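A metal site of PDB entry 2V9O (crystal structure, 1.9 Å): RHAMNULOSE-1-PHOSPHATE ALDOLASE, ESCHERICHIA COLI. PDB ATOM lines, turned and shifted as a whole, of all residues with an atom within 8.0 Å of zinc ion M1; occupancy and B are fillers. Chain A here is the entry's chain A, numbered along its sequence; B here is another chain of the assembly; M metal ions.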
ATOM      1  N   TRP A  25      -5.712 -32.350  -6.232  1.00  0.00           N
ATOM      2  CA  TRP A  25      -5.615 -30.902  -6.278  1.00  0.00           C
ATOM      3  C   TRP A  25      -5.838 -30.183  -4.979  1.00  0.00           C
ATOM      4  O   TRP A  25      -5.693 -28.980  -4.922  1.00  0.00           O
ATOM      5  CB  TRP A  25      -6.573 -30.287  -7.293  1.00  0.00           C
ATOM      6  CG  TRP A  25      -6.377 -30.829  -8.773  1.00  0.00           C
ATOM      7  CD1 TRP A  25      -5.363 -31.594  -9.271  1.00  0.00           C
ATOM      8  CD2 TRP A  25      -7.280 -30.567  -9.870  1.00  0.00           C
ATOM      9  NE1 TRP A  25      -5.615 -31.897 -10.627  1.00  0.00           N
ATOM     10  CE2 TRP A  25      -6.788 -31.273 -10.995  1.00  0.00           C
ATOM     11  CE3 TRP A  25      -8.522 -29.919  -9.957  1.00  0.00           C
ATOM     12  CZ2 TRP A  25      -7.463 -31.272 -12.232  1.00  0.00           C
ATOM     13  CZ3 TRP A  25      -9.204 -29.877 -11.214  1.00  0.00           C
ATOM     14  CH2 TRP A  25      -8.681 -30.563 -12.299  1.00  0.00           C
ATOM     15  N   ASP A  26      -6.227 -30.897  -3.931  1.00  0.00           N
ATOM     16  CA  ASP A  26      -6.776 -30.158  -2.817  1.00  0.00           C
ATOM     17  C   ASP A  26      -6.422 -30.857  -1.504  1.00  0.00           C
ATOM     18  O   ASP A  26      -7.280 -31.290  -0.746  1.00  0.00           O
ATOM     19  CB  ASP A  26      -8.249 -30.035  -3.052  1.00  0.00           C
ATOM     20  CG  ASP A  26      -8.592 -28.966  -4.125  1.00  0.00           C
ATOM     21  OD1 ASP A  26      -8.923 -29.348  -5.247  1.00  0.00           O
ATOM     22  OD2 ASP A  26      -8.506 -27.738  -3.821  1.00  0.00           O
ATOM     23  N   GLU A  27      -5.116 -31.033  -1.310  1.00  0.00           N
ATOM     24  CA  GLU A  27      -4.473 -31.541  -0.086  1.00  0.00           C
ATOM     25  C   GLU A  27      -4.955 -30.616   1.049  1.00  0.00           C
ATOM     26  O   GLU A  27      -5.211 -29.440   0.802  1.00  0.00           O
ATOM     27  CB  GLU A  27      -2.946 -31.454  -0.206  1.00  0.00           C
ATOM     28  CG  GLU A  27      -2.294 -29.982  -0.095  1.00  0.00           C
ATOM     29  CD  GLU A  27      -2.340 -29.159  -1.378  1.00  0.00           C
ATOM     30  OE1 GLU A  27      -1.840 -27.958  -1.404  1.00  0.00           O
ATOM     31  OE2 GLU A  27      -2.836 -29.736  -2.375  1.00  0.00           O
ATOM     32  N   ASN A  29      -6.699 -28.180   3.517  1.00  0.00           N
ATOM     33  CA  ASN A  29      -7.711 -27.173   3.060  1.00  0.00           C
ATOM     34  C   ASN A  29      -7.380 -26.460   1.767  1.00  0.00           C
ATOM     35  O   ASN A  29      -7.916 -25.342   1.552  1.00  0.00           O
ATOM     36  CB  ASN A  29      -7.899 -26.034   4.108  1.00  0.00           C
ATOM     37  CG  ASN A  29      -6.633 -25.337   4.446  1.00  0.00           C
ATOM     38  OD1 ASN A  29      -5.746 -25.941   5.037  1.00  0.00           O
ATOM     39  ND2 ASN A  29      -6.535 -24.038   4.117  1.00  0.00           N
ATOM     40  N   GLY A  30      -6.443 -26.996   0.990  1.00  0.00           N
ATOM     41  CA  GLY A  30      -5.927 -26.281  -0.160  1.00  0.00           C
ATOM     42  C   GLY A  30      -7.003 -26.066  -1.194  1.00  0.00           C
ATOM     43  O   GLY A  30      -7.720 -26.985  -1.548  1.00  0.00           O
ATOM     44  N   GLY A  31      -7.109 -24.878  -1.770  1.00  0.00           N
ATOM     45  CA  GLY A  31      -8.037 -24.738  -2.905  1.00  0.00           C
ATOM     46  C   GLY A  31      -9.276 -24.108  -2.312  1.00  0.00           C
ATOM     47  O   GLY A  31      -9.539 -24.231  -1.114  1.00  0.00           O
ATOM     48  N   ASN A  32     -10.085 -23.439  -3.120  1.00  0.00           N
ATOM     49  CA  ASN A  32     -11.366 -22.963  -2.636  1.00  0.00           C
ATOM     50  C   ASN A  32     -12.281 -22.673  -3.803  1.00  0.00           C
ATOM     51  O   ASN A  32     -11.808 -22.619  -4.897  1.00  0.00           O
ATOM     52  CB  ASN A  32     -11.134 -21.683  -1.778  1.00  0.00           C
ATOM     53  CG  ASN A  32      -9.756 -20.998  -2.099  1.00  0.00           C
ATOM     54  OD1 ASN A  32      -9.637 -20.249  -3.075  1.00  0.00           O
ATOM     55  ND2 ASN A  32      -8.714 -21.329  -1.274  1.00  0.00           N
ATOM     56  N   THR A 115     -13.898 -18.986   2.860  1.00  0.00           N
ATOM     57  CA  THR A 115     -12.481 -19.028   2.467  1.00  0.00           C
ATOM     58  C   THR A 115     -11.618 -17.781   2.686  1.00  0.00           C
ATOM     59  O   THR A 115     -12.062 -16.607   2.462  1.00  0.00           O
ATOM     60  CB  THR A 115     -12.314 -19.471   1.039  1.00  0.00           C
ATOM     61  OG1 THR A 115     -10.936 -19.669   0.784  1.00  0.00           O
ATOM     62  CG2 THR A 115     -12.931 -18.468   0.073  1.00  0.00           C
ATOM     63  N   SER A 116     -10.382 -18.031   3.140  1.00  0.00           N
ATOM     64  CA  SER A 116      -9.416 -16.944   3.369  1.00  0.00           C
ATOM     65  C   SER A 116      -8.957 -16.322   2.028  1.00  0.00           C
ATOM     66  O   SER A 116      -8.331 -15.251   2.038  1.00  0.00           O
ATOM     67  CB  SER A 116      -8.236 -17.448   4.203  1.00  0.00           C
ATOM     68  OG  SER A 116      -7.557 -18.396   3.408  1.00  0.00           O
ATOM     69  N   GLU A 117      -9.316 -16.936   0.897  1.00  0.00           N
ATOM     70  CA  GLU A 117      -9.064 -16.306  -0.402  1.00  0.00           C
ATOM     71  C   GLU A 117     -10.270 -15.539  -0.905  1.00  0.00           C
ATOM     72  O   GLU A 117     -10.306 -15.215  -2.080  1.00  0.00           O
ATOM     73  CB  GLU A 117      -8.615 -17.267  -1.505  1.00  0.00           C
ATOM     74  CG  GLU A 117      -7.365 -18.080  -1.189  1.00  0.00           C
ATOM     75  CD  GLU A 117      -6.107 -17.271  -1.177  1.00  0.00           C
ATOM     76  OE1 GLU A 117      -5.088 -17.941  -0.993  1.00  0.00           O
ATOM     77  OE2 GLU A 117      -6.116 -16.006  -1.345  1.00  0.00           O
ATOM     78  N   HIS A 141     -10.311 -22.229  -7.297  1.00  0.00           N
ATOM     79  CA  HIS A 141      -8.889 -22.249  -7.063  1.00  0.00           C
ATOM     80  C   HIS A 141      -8.547 -23.630  -6.552  1.00  0.00           C
ATOM     81  O   HIS A 141      -9.206 -24.164  -5.569  1.00  0.00           O
ATOM     82  CB  HIS A 141      -8.470 -21.164  -6.019  1.00  0.00           C
ATOM     83  CG  HIS A 141      -7.097 -21.354  -5.416  1.00  0.00           C
ATOM     84  ND1 HIS A 141      -5.954 -21.412  -6.177  1.00  0.00           N
ATOM     85  CD2 HIS A 141      -6.652 -21.397  -4.120  1.00  0.00           C
ATOM     86  CE1 HIS A 141      -4.886 -21.495  -5.398  1.00  0.00           C
ATOM     87  NE2 HIS A 141      -5.276 -21.474  -4.140  1.00  0.00           N
ATOM     88  N   CYS A 142      -7.543 -24.240  -7.202  1.00  0.00           N
ATOM     89  CA  CYS A 142      -7.041 -25.529  -6.698  1.00  0.00           C
ATOM     90  C   CYS A 142      -5.568 -25.656  -6.883  1.00  0.00           C
ATOM     91  O   CYS A 142      -4.998 -24.962  -7.662  1.00  0.00           O
ATOM     92  CB  CYS A 142      -7.706 -26.694  -7.453  1.00  0.00           C
ATOM     93  SG  CYS A 142      -7.512 -26.592  -9.212  1.00  0.00           S
ATOM     94  N   HIS A 143      -4.939 -26.562  -6.141  1.00  0.00           N
ATOM     95  CA  HIS A 143      -3.526 -26.710  -6.265  1.00  0.00           C
ATOM     96  C   HIS A 143      -3.211 -27.791  -7.342  1.00  0.00           C
ATOM     97  O   HIS A 143      -2.890 -28.931  -6.979  1.00  0.00           O
ATOM     98  CB  HIS A 143      -3.003 -27.088  -4.912  1.00  0.00           C
ATOM     99  CG  HIS A 143      -3.195 -25.991  -3.908  1.00  0.00           C
ATOM    100  ND1 HIS A 143      -2.861 -26.109  -2.579  1.00  0.00           N
ATOM    101  CD2 HIS A 143      -3.707 -24.757  -4.061  1.00  0.00           C
ATOM    102  CE1 HIS A 143      -3.096 -24.938  -1.966  1.00  0.00           C
ATOM    103  NE2 HIS A 143      -3.658 -24.141  -2.845  1.00  0.00           N
ATOM    104  N   ILE A 148       1.377 -26.496 -11.161  1.00  0.00           N
ATOM    105  CA  ILE A 148       2.227 -25.870 -10.151  1.00  0.00           C
ATOM    106  C   ILE A 148       3.702 -26.242 -10.542  1.00  0.00           C
ATOM    107  O   ILE A 148       4.627 -25.430 -10.447  1.00  0.00           O
ATOM    108  CB  ILE A 148       1.874 -26.519  -8.809  1.00  0.00           C
ATOM    109  CG1 ILE A 148       0.539 -26.013  -8.298  1.00  0.00           C
ATOM    110  CG2 ILE A 148       3.003 -26.285  -7.721  1.00  0.00           C
ATOM    111  CD1 ILE A 148      -0.012 -26.798  -7.057  1.00  0.00           C
ATOM    112  N   PRO A 188      -0.364 -15.105  -0.257  1.00  0.00           N
ATOM    113  CA  PRO A 188      -1.737 -15.405  -0.503  1.00  0.00           C
ATOM    114  C   PRO A 188      -2.658 -14.942   0.681  1.00  0.00           C
ATOM    115  O   PRO A 188      -2.147 -14.653   1.806  1.00  0.00           O
ATOM    116  CB  PRO A 188      -1.686 -16.901  -0.691  1.00  0.00           C
ATOM    117  CG  PRO A 188      -0.569 -17.358   0.214  1.00  0.00           C
ATOM    118  CD  PRO A 188       0.425 -16.318   0.126  1.00  0.00           C
ATOM    119  N   GLY A 189      -3.953 -14.764   0.371  1.00  0.00           N
ATOM    120  CA  GLY A 189      -5.003 -14.610   1.335  1.00  0.00           C
ATOM    121  C   GLY A 189      -5.046 -13.147   1.729  1.00  0.00           C
ATOM    122  O   GLY A 189      -5.514 -12.843   2.834  1.00  0.00           O
ATOM    123  N   TRP A 209      -0.870 -18.748 -10.029  1.00  0.00           N
ATOM    124  CA  TRP A 209      -0.139 -18.305  -8.911  1.00  0.00           C
ATOM    125  C   TRP A 209       1.033 -19.232  -8.888  1.00  0.00           C
ATOM    126  O   TRP A 209       0.879 -20.350  -8.400  1.00  0.00           O
ATOM    127  CB  TRP A 209      -1.005 -18.532  -7.667  1.00  0.00           C
ATOM    128  CG  TRP A 209      -2.138 -17.521  -7.521  1.00  0.00           C
ATOM    129  CD1 TRP A 209      -2.611 -16.629  -8.477  1.00  0.00           C
ATOM    130  CD2 TRP A 209      -2.964 -17.352  -6.384  1.00  0.00           C
ATOM    131  NE1 TRP A 209      -3.618 -15.937  -7.983  1.00  0.00           N
ATOM    132  CE2 TRP A 209      -3.841 -16.314  -6.686  1.00  0.00           C
ATOM    133  CE3 TRP A 209      -3.009 -17.937  -5.114  1.00  0.00           C
ATOM    134  CZ2 TRP A 209      -4.769 -15.831  -5.774  1.00  0.00           C
ATOM    135  CZ3 TRP A 209      -3.941 -17.433  -4.197  1.00  0.00           C
ATOM    136  CH2 TRP A 209      -4.795 -16.414  -4.541  1.00  0.00           C
ATOM    137  N   PHE A 211       4.023 -21.520  -8.009  1.00  0.00           N
ATOM    138  CA  PHE A 211       4.468 -22.230  -6.814  1.00  0.00           C
ATOM    139  C   PHE A 211       3.288 -22.343  -5.829  1.00  0.00           C
ATOM    140  O   PHE A 211       3.456 -22.620  -4.652  1.00  0.00           O
ATOM    141  CB  PHE A 211       5.719 -21.613  -6.126  1.00  0.00           C
ATOM    142  CG  PHE A 211       6.675 -20.861  -7.069  1.00  0.00           C
ATOM    143  CD1 PHE A 211       7.064 -19.550  -6.778  1.00  0.00           C
ATOM    144  CD2 PHE A 211       7.197 -21.470  -8.220  1.00  0.00           C
ATOM    145  CE1 PHE A 211       7.900 -18.828  -7.647  1.00  0.00           C
ATOM    146  CE2 PHE A 211       8.069 -20.768  -9.097  1.00  0.00           C
ATOM    147  CZ  PHE A 211       8.387 -19.433  -8.803  1.00  0.00           C
ATOM    148  N   HIS A 212       2.092 -22.223  -6.394  1.00  0.00           N
ATOM    149  CA  HIS A 212       0.924 -22.328  -5.550  1.00  0.00           C
ATOM    150  C   HIS A 212      -0.312 -22.995  -6.174  1.00  0.00           C
ATOM    151  O   HIS A 212      -0.733 -24.096  -5.769  1.00  0.00           O
ATOM    152  CB  HIS A 212       0.573 -20.888  -5.203  1.00  0.00           C
ATOM    153  CG  HIS A 212      -0.493 -20.779  -4.196  1.00  0.00           C
ATOM    154  ND1 HIS A 212      -0.595 -19.715  -3.298  1.00  0.00           N
ATOM    155  CD2 HIS A 212      -1.601 -21.523  -4.049  1.00  0.00           C
ATOM    156  CE1 HIS A 212      -1.677 -19.907  -2.557  1.00  0.00           C
ATOM    157  NE2 HIS A 212      -2.277 -21.026  -2.980  1.00  0.00           N
ATOM    158  N   GLY A 213      -0.951 -22.294  -7.125  1.00  0.00           N
ATOM    159  CA  GLY A 213      -2.033 -22.974  -7.848  1.00  0.00           C
ATOM    160  C   GLY A 213      -2.576 -22.242  -9.053  1.00  0.00           C
ATOM    161  O   GLY A 213      -1.855 -21.443  -9.644  1.00  0.00           O
ATOM    162  N   VAL A 214      -3.820 -22.543  -9.430  1.00  0.00           N
ATOM    163  CA  VAL A 214      -4.493 -21.887 -10.536  1.00  0.00           C
ATOM    164  C   VAL A 214      -5.873 -21.425 -10.033  1.00  0.00           C
ATOM    165  O   VAL A 214      -6.421 -21.970  -9.054  1.00  0.00           O
ATOM    166  CB  VAL A 214      -4.569 -22.805 -11.719  1.00  0.00           C
ATOM    167  CG1 VAL A 214      -5.500 -23.979 -11.410  1.00  0.00           C
ATOM    168  CG2 VAL A 214      -5.009 -22.153 -13.004  1.00  0.00           C
ATOM    169  N   PHE A 215      -6.366 -20.372 -10.656  1.00  0.00           N
ATOM    170  CA  PHE A 215      -7.656 -19.766 -10.457  1.00  0.00           C
ATOM    171  C   PHE A 215      -8.281 -19.866 -11.842  1.00  0.00           C
ATOM    172  O   PHE A 215      -7.586 -19.633 -12.829  1.00  0.00           O
ATOM    173  CB  PHE A 215      -7.533 -18.289 -10.049  1.00  0.00           C
ATOM    174  CG  PHE A 215      -7.666 -18.064  -8.601  1.00  0.00           C
ATOM    175  CD1 PHE A 215      -6.618 -18.318  -7.762  1.00  0.00           C
ATOM    176  CD2 PHE A 215      -8.867 -17.699  -8.041  1.00  0.00           C
ATOM    177  CE1 PHE A 215      -6.769 -18.124  -6.355  1.00  0.00           C
ATOM    178  CE2 PHE A 215      -9.001 -17.585  -6.678  1.00  0.00           C
ATOM    179  CZ  PHE A 215      -7.988 -17.782  -5.830  1.00  0.00           C
ATOM    180  N   THR B 170       3.327 -23.389  -1.862  1.00  0.00           N
ATOM    181  CA  THR B 170       3.339 -22.193  -1.038  1.00  0.00           C
ATOM    182  C   THR B 170       2.914 -22.300   0.419  1.00  0.00           C
ATOM    183  O   THR B 170       3.512 -21.670   1.313  1.00  0.00           O
ATOM    184  CB  THR B 170       2.557 -21.049  -1.661  1.00  0.00           C
ATOM    185  OG1 THR B 170       3.281 -20.576  -2.812  1.00  0.00           O
ATOM    186  CG2 THR B 170       2.471 -19.877  -0.674  1.00  0.00           C
ATOM    187  N   GLU B 171       1.831 -23.051   0.657  1.00  0.00           N
ATOM    188  CA  GLU B 171       1.162 -23.239   1.928  1.00  0.00           C
ATOM    189  C   GLU B 171       1.954 -23.997   2.983  1.00  0.00           C
ATOM    190  O   GLU B 171       1.545 -24.120   4.084  1.00  0.00           O
ATOM    191  CB  GLU B 171      -0.058 -24.086   1.572  1.00  0.00           C
ATOM    192  CG  GLU B 171       0.078 -24.917   0.223  1.00  0.00           C
ATOM    193  CD  GLU B 171      -0.339 -26.362   0.386  1.00  0.00           C
ATOM    194  OE1 GLU B 171      -1.496 -26.645   0.738  1.00  0.00           O
ATOM    195  OE2 GLU B 171       0.495 -27.247   0.178  1.00  0.00           O
HETATM  196 ZN    ZN M   1      -4.173 -22.001  -2.487  1.00  0.00          ZN
HETATM  197 ZN    ZN M   2      -8.981 -21.876   2.589  1.00  0.00          ZN
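The backbone carbonyl oxygen of His 141 is in hydrogen-bond range of the backbone NH of Asn 32 (2.7 Å).
ND1 of His 141 lies within hydrogen-bond range of O of Val 214 (3.0 Å).
A ring nitrogen (ND1) of His 143 is in hydrogen-bond range of the side-chain carboxylate (OE1) of Glu 27 (2.4 Å).
The backbone NH of His 143 is in hydrogen-bond range of the backbone carbonyl oxygen of Trp 25 (2.8 Å).
Of the 24 residues printed, 3 come within 4 Å of zinc ion M1.
Zinc ion M1 is bound by a ring nitrogen (NE2) of His 141, at 2.1 Å.
NE2 of His 212 binds zinc ion M1, at 2.2 Å.
NE2 of His 143 binds zinc ion M1 (2.2 Å).
Zinc ion M1 has three donor atoms within binding distance.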
